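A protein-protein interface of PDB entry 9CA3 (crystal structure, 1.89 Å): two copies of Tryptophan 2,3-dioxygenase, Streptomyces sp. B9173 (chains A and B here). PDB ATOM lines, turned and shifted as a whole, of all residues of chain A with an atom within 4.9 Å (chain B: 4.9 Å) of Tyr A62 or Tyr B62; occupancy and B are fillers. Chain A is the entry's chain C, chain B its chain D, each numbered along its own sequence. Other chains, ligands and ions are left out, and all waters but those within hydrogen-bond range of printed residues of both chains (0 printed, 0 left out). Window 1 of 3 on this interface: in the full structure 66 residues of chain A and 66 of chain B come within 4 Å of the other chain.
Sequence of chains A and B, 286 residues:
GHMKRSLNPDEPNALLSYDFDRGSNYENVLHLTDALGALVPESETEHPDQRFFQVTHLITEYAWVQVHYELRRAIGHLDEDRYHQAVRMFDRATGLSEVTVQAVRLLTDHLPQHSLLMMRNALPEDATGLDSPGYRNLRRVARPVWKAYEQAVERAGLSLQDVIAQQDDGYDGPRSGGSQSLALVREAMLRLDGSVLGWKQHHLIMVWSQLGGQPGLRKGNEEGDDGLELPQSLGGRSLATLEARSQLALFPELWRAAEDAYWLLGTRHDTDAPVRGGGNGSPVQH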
ATOM      1  N   ALA A  35       9.683 -24.410  11.041  1.00  0.00           N
ATOM      2  CA  ALA A  35       9.862 -23.067  10.500  1.00  0.00           C
ATOM      3  C   ALA A  35       8.651 -22.191  10.795  1.00  0.00           C
ATOM      4  O   ALA A  35       8.800 -21.005  11.122  1.00  0.00           O
ATOM      5  CB  ALA A  35      10.138 -23.136   8.994  1.00  0.00           C
ATOM      6  N   LEU A  36       7.443 -22.762  10.704  1.00  0.00           N
ATOM      7  CA  LEU A  36       6.230 -22.006  11.029  1.00  0.00           C
ATOM      8  C   LEU A  36       6.159 -21.661  12.514  1.00  0.00           C
ATOM      9  O   LEU A  36       5.542 -20.655  12.885  1.00  0.00           O
ATOM     10  CB  LEU A  36       4.988 -22.813  10.616  1.00  0.00           C
ATOM     11  CG  LEU A  36       4.768 -22.943   9.102  1.00  0.00           C
ATOM     12  CD1 LEU A  36       3.563 -23.798   8.734  1.00  0.00           C
ATOM     13  CD2 LEU A  36       4.660 -21.558   8.477  1.00  0.00           C
ATOM     14  N   ALA A  38       8.450 -20.478  14.264  1.00  0.00           N
ATOM     15  CA  ALA A  38       9.166 -19.242  14.527  1.00  0.00           C
ATOM     16  C   ALA A  38       8.247 -18.027  14.481  1.00  0.00           C
ATOM     17  O   ALA A  38       8.614 -16.971  15.001  1.00  0.00           O
ATOM     18  CB  ALA A  38      10.320 -19.089  13.518  1.00  0.00           C
ATOM     19  N   LEU A  39       7.070 -18.147  13.871  1.00  0.00           N
ATOM     20  CA  LEU A  39       6.170 -17.002  13.774  1.00  0.00           C
ATOM     21  C   LEU A  39       5.704 -16.576  15.160  1.00  0.00           C
ATOM     22  O   LEU A  39       5.391 -17.415  16.015  1.00  0.00           O
ATOM     23  CB  LEU A  39       4.968 -17.339  12.895  1.00  0.00           C
ATOM     24  CG  LEU A  39       5.299 -17.575  11.414  1.00  0.00           C
ATOM     25  CD1 LEU A  39       4.049 -17.986  10.683  1.00  0.00           C
ATOM     26  CD2 LEU A  39       5.903 -16.303  10.778  1.00  0.00           C
ATOM     27  N   VAL A  55       7.570 -11.443   8.896  1.00  0.00           N
ATOM     28  CA  VAL A  55       7.687 -12.383   7.789  1.00  0.00           C
ATOM     29  C   VAL A  55       8.606 -11.827   6.703  1.00  0.00           C
ATOM     30  O   VAL A  55       9.434 -12.553   6.170  1.00  0.00           O
ATOM     31  CB  VAL A  55       6.292 -12.773   7.252  1.00  0.00           C
ATOM     32  CG1 VAL A  55       6.383 -13.442   5.901  1.00  0.00           C
ATOM     33  CG2 VAL A  55       5.643 -13.740   8.225  1.00  0.00           C
ATOM     34  N   LEU A  58      12.055 -12.594   7.794  1.00  0.00           N
ATOM     35  CA  LEU A  58      12.384 -14.010   7.740  1.00  0.00           C
ATOM     36  C   LEU A  58      12.601 -14.479   6.310  1.00  0.00           C
ATOM     37  O   LEU A  58      13.480 -15.294   6.055  1.00  0.00           O
ATOM     38  CB  LEU A  58      11.297 -14.835   8.411  1.00  0.00           C
ATOM     39  CG  LEU A  58      11.150 -14.665   9.917  1.00  0.00           C
ATOM     40  CD1 LEU A  58      10.117 -15.672  10.413  1.00  0.00           C
ATOM     41  CD2 LEU A  58      12.462 -14.837  10.639  1.00  0.00           C
ATOM     42  N   ILE A  59      11.796 -14.007   5.367  1.00  0.00           N
ATOM     43  CA  ILE A  59      12.046 -14.360   3.971  1.00  0.00           C
ATOM     44  C   ILE A  59      13.429 -13.887   3.552  1.00  0.00           C
ATOM     45  O   ILE A  59      14.184 -14.609   2.889  1.00  0.00           O
ATOM     46  CB  ILE A  59      10.935 -13.761   3.089  1.00  0.00           C
ATOM     47  CG1 ILE A  59       9.633 -14.565   3.310  1.00  0.00           C
ATOM     48  CG2 ILE A  59      11.372 -13.693   1.611  1.00  0.00           C
ATOM     49  CD1 ILE A  59       8.386 -13.892   2.777  1.00  0.00           C
ATOM     50  N   THR A  60      13.793 -12.672   3.964  1.00  0.00           N
ATOM     51  CA  THR A  60      15.089 -12.122   3.594  1.00  0.00           C
ATOM     52  C   THR A  60      16.217 -12.955   4.171  1.00  0.00           C
ATOM     53  O   THR A  60      17.166 -13.301   3.462  1.00  0.00           O
ATOM     54  CB  THR A  60      15.203 -10.676   4.089  1.00  0.00           C
ATOM     55  OG1 THR A  60      14.099  -9.900   3.586  1.00  0.00           O
ATOM     56  CG2 THR A  60      16.515 -10.057   3.642  1.00  0.00           C
ATOM     57  N   GLU A  61      16.132 -13.302   5.461  1.00  0.00           N
ATOM     58  CA  GLU A  61      17.240 -14.074   6.037  1.00  0.00           C
ATOM     59  C   GLU A  61      17.325 -15.484   5.471  1.00  0.00           C
ATOM     60  O   GLU A  61      18.430 -16.042   5.392  1.00  0.00           O
ATOM     61  CB  GLU A  61      17.131 -14.117   7.556  1.00  0.00           C
ATOM     62  CG  GLU A  61      17.149 -12.716   8.161  1.00  0.00           C
ATOM     63  CD  GLU A  61      18.572 -12.219   8.362  1.00  0.00           C
ATOM     64  OE1 GLU A  61      19.496 -13.025   8.124  1.00  0.00           O
ATOM     65  OE2 GLU A  61      18.774 -11.032   8.726  1.00  0.00           O
ATOM     66  N   TYR A  62      16.198 -16.099   5.088  1.00  0.00           N
ATOM     67  CA  TYR A  62      16.304 -17.376   4.376  1.00  0.00           C
ATOM     68  C   TYR A  62      17.040 -17.198   3.051  1.00  0.00           C
ATOM     69  O   TYR A  62      17.932 -17.985   2.705  1.00  0.00           O
ATOM     70  CB  TYR A  62      14.917 -17.980   4.123  1.00  0.00           C
ATOM     71  CG  TYR A  62      14.407 -18.882   5.225  1.00  0.00           C
ATOM     72  CD1 TYR A  62      15.279 -19.480   6.136  1.00  0.00           C
ATOM     73  CD2 TYR A  62      13.051 -19.135   5.358  1.00  0.00           C
ATOM     74  CE1 TYR A  62      14.805 -20.314   7.158  1.00  0.00           C
ATOM     75  CE2 TYR A  62      12.580 -19.956   6.352  1.00  0.00           C
ATOM     76  CZ  TYR A  62      13.451 -20.545   7.255  1.00  0.00           C
ATOM     77  OH  TYR A  62      12.916 -21.341   8.257  1.00  0.00           O
ATOM     78  N   ALA A  63      16.674 -16.156   2.289  1.00  0.00           N
ATOM     79  CA  ALA A  63      17.321 -15.926   1.000  1.00  0.00           C
ATOM     80  C   ALA A  63      18.821 -15.681   1.174  1.00  0.00           C
ATOM     81  O   ALA A  63      19.630 -16.247   0.441  1.00  0.00           O
ATOM     82  CB  ALA A  63      16.648 -14.758   0.274  1.00  0.00           C
ATOM     83  N   TRP A  64      19.212 -14.903   2.192  1.00  0.00           N
ATOM     84  CA  TRP A  64      20.628 -14.581   2.374  1.00  0.00           C
ATOM     85  C   TRP A  64      21.431 -15.802   2.838  1.00  0.00           C
ATOM     86  O   TRP A  64      22.596 -15.968   2.447  1.00  0.00           O
ATOM     87  CB  TRP A  64      20.781 -13.433   3.375  1.00  0.00           C
ATOM     88  CG  TRP A  64      20.654 -12.078   2.764  1.00  0.00           C
ATOM     89  CD1 TRP A  64      20.797 -11.761   1.441  1.00  0.00           C
ATOM     90  CD2 TRP A  64      20.337 -10.858   3.439  1.00  0.00           C
ATOM     91  NE1 TRP A  64      20.605 -10.407   1.256  1.00  0.00           N
ATOM     92  CE2 TRP A  64      20.324  -9.830   2.465  1.00  0.00           C
ATOM     93  CE3 TRP A  64      20.071 -10.527   4.776  1.00  0.00           C
ATOM     94  CZ2 TRP A  64      20.060  -8.486   2.785  1.00  0.00           C
ATOM     95  CZ3 TRP A  64      19.791  -9.194   5.091  1.00  0.00           C
ATOM     96  CH2 TRP A  64      19.798  -8.193   4.097  1.00  0.00           C
ATOM     97  N   VAL A  65      20.845 -16.671   3.678  1.00  0.00           N
ATOM     98  CA  VAL A  65      21.647 -17.829   4.066  1.00  0.00           C
ATOM     99  C   VAL A  65      21.845 -18.752   2.866  1.00  0.00           C
ATOM    100  O   VAL A  65      22.850 -19.464   2.778  1.00  0.00           O
ATOM    101  CB  VAL A  65      21.052 -18.572   5.282  1.00  0.00           C
ATOM    102  CG1 VAL A  65      19.744 -19.295   4.930  1.00  0.00           C
ATOM    103  CG2 VAL A  65      22.087 -19.604   5.817  1.00  0.00           C
ATOM    104  N   GLN A  66      20.899 -18.757   1.925  1.00  0.00           N
ATOM    105  CA  GLN A  66      21.076 -19.539   0.715  1.00  0.00           C
ATOM    106  C   GLN A  66      22.087 -18.862  -0.214  1.00  0.00           C
ATOM    107  O   GLN A  66      22.919 -19.547  -0.833  1.00  0.00           O
ATOM    108  CB  GLN A  66      19.723 -19.774   0.030  1.00  0.00           C
ATOM    109  CG  GLN A  66      19.720 -20.937  -0.987  1.00  0.00           C
ATOM    110  CD  GLN A  66      20.264 -22.228  -0.397  1.00  0.00           C
ATOM    111  OE1 GLN A  66      19.934 -22.576   0.728  1.00  0.00           O
ATOM    112  NE2 GLN A  66      21.101 -22.951  -1.166  1.00  0.00           N
ATOM    113  N   ALA B  35      13.829 -20.082  13.183  1.00  0.00           N
ATOM    114  CA  ALA B  35      13.619 -20.245  11.742  1.00  0.00           C
ATOM    115  C   ALA B  35      14.843 -20.859  11.056  1.00  0.00           C
ATOM    116  O   ALA B  35      14.724 -21.774  10.222  1.00  0.00           O
ATOM    117  CB  ALA B  35      13.262 -18.889  11.127  1.00  0.00           C
ATOM    118  N   LEU B  36      16.034 -20.355  11.381  1.00  0.00           N
ATOM    119  CA  LEU B  36      17.248 -20.942  10.831  1.00  0.00           C
ATOM    120  C   LEU B  36      17.409 -22.387  11.294  1.00  0.00           C
ATOM    121  O   LEU B  36      17.960 -23.222  10.559  1.00  0.00           O
ATOM    122  CB  LEU B  36      18.456 -20.093  11.242  1.00  0.00           C
ATOM    123  CG  LEU B  36      18.541 -18.698  10.589  1.00  0.00           C
ATOM    124  CD1 LEU B  36      19.757 -17.883  11.098  1.00  0.00           C
ATOM    125  CD2 LEU B  36      18.551 -18.795   9.070  1.00  0.00           C
ATOM    126  N   ALA B  38      15.298 -24.598  11.294  1.00  0.00           N
ATOM    127  CA  ALA B  38      14.546 -25.519  10.456  1.00  0.00           C
ATOM    128  C   ALA B  38      15.303 -25.954   9.204  1.00  0.00           C
ATOM    129  O   ALA B  38      14.841 -26.856   8.502  1.00  0.00           O
ATOM    130  CB  ALA B  38      13.200 -24.897  10.063  1.00  0.00           C
ATOM    131  N   LEU B  39      16.448 -25.352   8.900  1.00  0.00           N
ATOM    132  CA  LEU B  39      17.176 -25.737   7.701  1.00  0.00           C
ATOM    133  C   LEU B  39      17.781 -27.128   7.890  1.00  0.00           C
ATOM    134  O   LEU B  39      18.261 -27.451   8.980  1.00  0.00           O
ATOM    135  CB  LEU B  39      18.272 -24.711   7.396  1.00  0.00           C
ATOM    136  CG  LEU B  39      17.782 -23.282   7.129  1.00  0.00           C
ATOM    137  CD1 LEU B  39      18.965 -22.304   6.988  1.00  0.00           C
ATOM    138  CD2 LEU B  39      16.875 -23.256   5.900  1.00  0.00           C
ATOM    139  N   VAL B  55      14.810 -24.084   0.784  1.00  0.00           N
ATOM    140  CA  VAL B  55      14.593 -22.673   1.088  1.00  0.00           C
ATOM    141  C   VAL B  55      13.521 -22.088   0.180  1.00  0.00           C
ATOM    142  O   VAL B  55      12.714 -21.256   0.606  1.00  0.00           O
ATOM    143  CB  VAL B  55      15.931 -21.905   0.949  1.00  0.00           C
ATOM    144  CG1 VAL B  55      15.683 -20.413   0.865  1.00  0.00           C
ATOM    145  CG2 VAL B  55      16.833 -22.212   2.107  1.00  0.00           C
ATOM    146  N   LEU B  58      10.304 -22.973   1.797  1.00  0.00           N
ATOM    147  CA  LEU B  58      10.071 -22.263   3.054  1.00  0.00           C
ATOM    148  C   LEU B  58       9.720 -20.799   2.810  1.00  0.00           C
ATOM    149  O   LEU B  58       8.866 -20.224   3.497  1.00  0.00           O
ATOM    150  CB  LEU B  58      11.308 -22.365   3.937  1.00  0.00           C
ATOM    151  CG  LEU B  58      11.685 -23.762   4.430  1.00  0.00           C
ATOM    152  CD1 LEU B  58      12.780 -23.666   5.478  1.00  0.00           C
ATOM    153  CD2 LEU B  58      10.462 -24.423   5.009  1.00  0.00           C
ATOM    154  N   ILE B  59      10.390 -20.168   1.852  1.00  0.00           N
ATOM    155  CA  ILE B  59      10.032 -18.799   1.500  1.00  0.00           C
ATOM    156  C   ILE B  59       8.596 -18.753   0.998  1.00  0.00           C
ATOM    157  O   ILE B  59       7.821 -17.861   1.358  1.00  0.00           O
ATOM    158  CB  ILE B  59      11.031 -18.244   0.468  1.00  0.00           C
ATOM    159  CG1 ILE B  59      12.341 -17.871   1.157  1.00  0.00           C
ATOM    160  CG2 ILE B  59      10.454 -17.031  -0.268  1.00  0.00           C
ATOM    161  CD1 ILE B  59      13.522 -17.587   0.178  1.00  0.00           C
ATOM    162  N   THR B  60       8.211 -19.728   0.181  1.00  0.00           N
ATOM    163  CA  THR B  60       6.860 -19.729  -0.353  1.00  0.00           C
ATOM    164  C   THR B  60       5.842 -19.849   0.767  1.00  0.00           C
ATOM    165  O   THR B  60       4.833 -19.132   0.790  1.00  0.00           O
ATOM    166  CB  THR B  60       6.665 -20.879  -1.335  1.00  0.00           C
ATOM    167  OG1 THR B  60       7.579 -20.731  -2.437  1.00  0.00           O
ATOM    168  CG2 THR B  60       5.213 -20.846  -1.847  1.00  0.00           C
ATOM    169  N   GLU B  61       6.092 -20.775   1.697  1.00  0.00           N
ATOM    170  CA  GLU B  61       5.137 -21.048   2.754  1.00  0.00           C
ATOM    171  C   GLU B  61       5.015 -19.867   3.705  1.00  0.00           C
ATOM    172  O   GLU B  61       3.934 -19.633   4.224  1.00  0.00           O
ATOM    173  CB  GLU B  61       5.515 -22.322   3.520  1.00  0.00           C
ATOM    174  CG  GLU B  61       5.396 -23.625   2.697  1.00  0.00           C
ATOM    175  CD  GLU B  61       3.958 -24.083   2.417  1.00  0.00           C
ATOM    176  OE1 GLU B  61       3.015 -23.567   3.042  1.00  0.00           O
ATOM    177  OE2 GLU B  61       3.778 -24.968   1.549  1.00  0.00           O
ATOM    178  N   TYR B  62       6.117 -19.142   3.959  1.00  0.00           N
ATOM    179  CA  TYR B  62       6.045 -17.924   4.753  1.00  0.00           C
ATOM    180  C   TYR B  62       5.184 -16.878   4.046  1.00  0.00           C
ATOM    181  O   TYR B  62       4.354 -16.217   4.678  1.00  0.00           O
ATOM    182  CB  TYR B  62       7.457 -17.367   5.006  1.00  0.00           C
ATOM    183  CG  TYR B  62       8.142 -17.922   6.237  1.00  0.00           C
ATOM    184  CD1 TYR B  62       7.412 -18.518   7.249  1.00  0.00           C
ATOM    185  CD2 TYR B  62       9.518 -17.849   6.387  1.00  0.00           C
ATOM    186  CE1 TYR B  62       8.022 -19.030   8.381  1.00  0.00           C
ATOM    187  CE2 TYR B  62      10.135 -18.361   7.527  1.00  0.00           C
ATOM    188  CZ  TYR B  62       9.370 -18.953   8.515  1.00  0.00           C
ATOM    189  OH  TYR B  62       9.971 -19.450   9.641  1.00  0.00           O
ATOM    190  N   ALA B  63       5.333 -16.738   2.721  1.00  0.00           N
ATOM    191  CA  ALA B  63       4.510 -15.740   2.046  1.00  0.00           C
ATOM    192  C   ALA B  63       3.041 -16.120   2.091  1.00  0.00           C
ATOM    193  O   ALA B  63       2.182 -15.249   2.295  1.00  0.00           O
ATOM    194  CB  ALA B  63       4.957 -15.543   0.604  1.00  0.00           C
ATOM    195  N   TRP B  64       2.733 -17.422   1.946  1.00  0.00           N
ATOM    196  CA  TRP B  64       1.334 -17.863   1.926  1.00  0.00           C
ATOM    197  C   TRP B  64       0.679 -17.781   3.305  1.00  0.00           C
ATOM    198  O   TRP B  64      -0.515 -17.472   3.407  1.00  0.00           O
ATOM    199  CB  TRP B  64       1.219 -19.303   1.403  1.00  0.00           C
ATOM    200  CG  TRP B  64       1.170 -19.378  -0.067  1.00  0.00           C
ATOM    201  CD1 TRP B  64       0.838 -18.368  -0.913  1.00  0.00           C
ATOM    202  CD2 TRP B  64       1.503 -20.505  -0.887  1.00  0.00           C
ATOM    203  NE1 TRP B  64       0.937 -18.792  -2.223  1.00  0.00           N
ATOM    204  CE2 TRP B  64       1.337 -20.102  -2.232  1.00  0.00           C
ATOM    205  CE3 TRP B  64       1.907 -21.818  -0.616  1.00  0.00           C
ATOM    206  CZ2 TRP B  64       1.561 -20.961  -3.305  1.00  0.00           C
ATOM    207  CZ3 TRP B  64       2.151 -22.678  -1.687  1.00  0.00           C
ATOM    208  CH2 TRP B  64       1.964 -22.247  -3.013  1.00  0.00           C
ATOM    209  N   VAL B  65       1.400 -18.106   4.382  1.00  0.00           N
ATOM    210  CA  VAL B  65       0.763 -17.911   5.689  1.00  0.00           C
ATOM    211  C   VAL B  65       0.498 -16.424   5.937  1.00  0.00           C
ATOM    212  O   VAL B  65      -0.500 -16.055   6.581  1.00  0.00           O
ATOM    213  CB  VAL B  65       1.594 -18.532   6.839  1.00  0.00           C
ATOM    214  CG1 VAL B  65       2.936 -17.805   7.016  1.00  0.00           C
ATOM    215  CG2 VAL B  65       0.789 -18.451   8.158  1.00  0.00           C
ATOM    216  N   GLN B  66       1.365 -15.544   5.419  1.00  0.00           N
ATOM    217  CA  GLN B  66       1.089 -14.116   5.547  1.00  0.00           C
ATOM    218  C   GLN B  66      -0.097 -13.712   4.676  1.00  0.00           C
ATOM    219  O   GLN B  66      -0.929 -12.903   5.090  1.00  0.00           O
ATOM    220  CB  GLN B  66       2.330 -13.276   5.196  1.00  0.00           C
ATOM    221  CG  GLN B  66       2.204 -11.820   5.729  1.00  0.00           C
ATOM    222  CD  GLN B  66       1.906 -11.756   7.223  1.00  0.00           C
ATOM    223  OE1 GLN B  66       2.503 -12.509   8.017  1.00  0.00           O
ATOM    224  NE2 GLN B  66       0.977 -10.849   7.629  1.00  0.00           N
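The backbone carbonyl oxygen (O) of Ala A35 sits at hydrogen-bond distance from the side-chain hydroxyl (OH) of Tyr B62 (2.4 Å).
O of Ala B35 is in hydrogen-bond range of OH of Tyr A62, 2.7 Å away.
Among the printed residues, pairs that only touch across the chains: Tyr A62 with Tyr B62 (3.1 Å), Val A55 with Gln B66 (3.4 Å), Gln A66 with Val B55 (3.4 Å), Tyr A62 with Leu B58 (3.6 Å), Val A55 with Tyr B62 (3.6 Å), Ala A38 with Ala B35 (3.7 Å), Ala A35 with Ala B38 (3.7 Å), Val A65 with Leu B39 (3.7 Å), Tyr A62 with Val B55 (3.8 Å), Tyr A62 with Leu B39 (3.8 Å), Leu A58 with Tyr B62 (3.8 Å), Leu A39 with Val B65 (3.8 Å), Ala A38 with Tyr B62 (3.9 Å), Tyr A62 with Ile B59 (3.9 Å), Ile A59 with Tyr B62 (3.9 Å), Ile A59 with Ile B59 (3.9 Å) and Tyr A62 with Ala B38 (3.998 Å).
Printed residues of chain B within 4 Å of Tyr A62: Ala B35, Ala B38, Leu B39, Val B55, Leu B58, Ile B59 and Tyr B62.
Printed residues of chain A within 4 Å of Leu B39: Tyr A62 (3.8 Å) and Val A65 (3.7 Å).
Printed residues of chain A within 4 Å of Val B55: Tyr A62 and Gln A66.
Tyr B62 touches just these residues of chain A: Ala A35 (2.4 Å), Ala A38 (3.9 Å), Val A55 (3.6 Å), Leu A58 (3.8 Å), Ile A59 (3.9 Å) and Tyr A62 (3.1 Å).
The nearest printed residue of chain B that does not touch Tyr A62 is Leu B36 (4.4 Å).
The nearest printed residue of chain A that does not touch Tyr B62 is Leu A39 (4.2 Å).
The nearest printed residue of chain B that does not touch Val A65 is Leu B36 (4.3 Å).
Hydrophobic or aromatic side chains of chain A that line the printed part of chain B: Ala A35, Ala A38, Leu A39, Val A55, Leu A58, Ile A59, Tyr A62 and Val A65.
Of the 14 printed residues of chain B, 9 touch a printed residue of chain A.
Hydrophobic or aromatic side chains of chain B within 4 Å of the printed part of chain A: Ala B35, Ala B38, Leu B39, Val B55, Leu B58, Ile B59, Tyr B62 and Val B65.
Among the printed residues, 19 pairs touch across the chains.
Among the printed residues, no Asp or Glu carboxylate lies within 4 Å of a Lys or Arg side-chain nitrogen of the other chain.
Ala A35 touches Ala B38, and with the chains exchanged Ala A38 touches Ala B35.
Ala A35 touches Tyr B62, and with the chains exchanged Tyr A62 touches Ala B35.
Val A55 touches Gln B66, and with the chains exchanged Gln A66 touches Val B55.
Tyr A62 touches its own counterpart, Tyr B62.
Positions printed for both chains: 35, 36, 38, 39, 55, 58, 59, 60, 61, 62, 63, 64, 65 and 66.
Of the 19 pairs that touch across the chains among the printed residues, 18 have their exchanged pair printed and touching as well.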
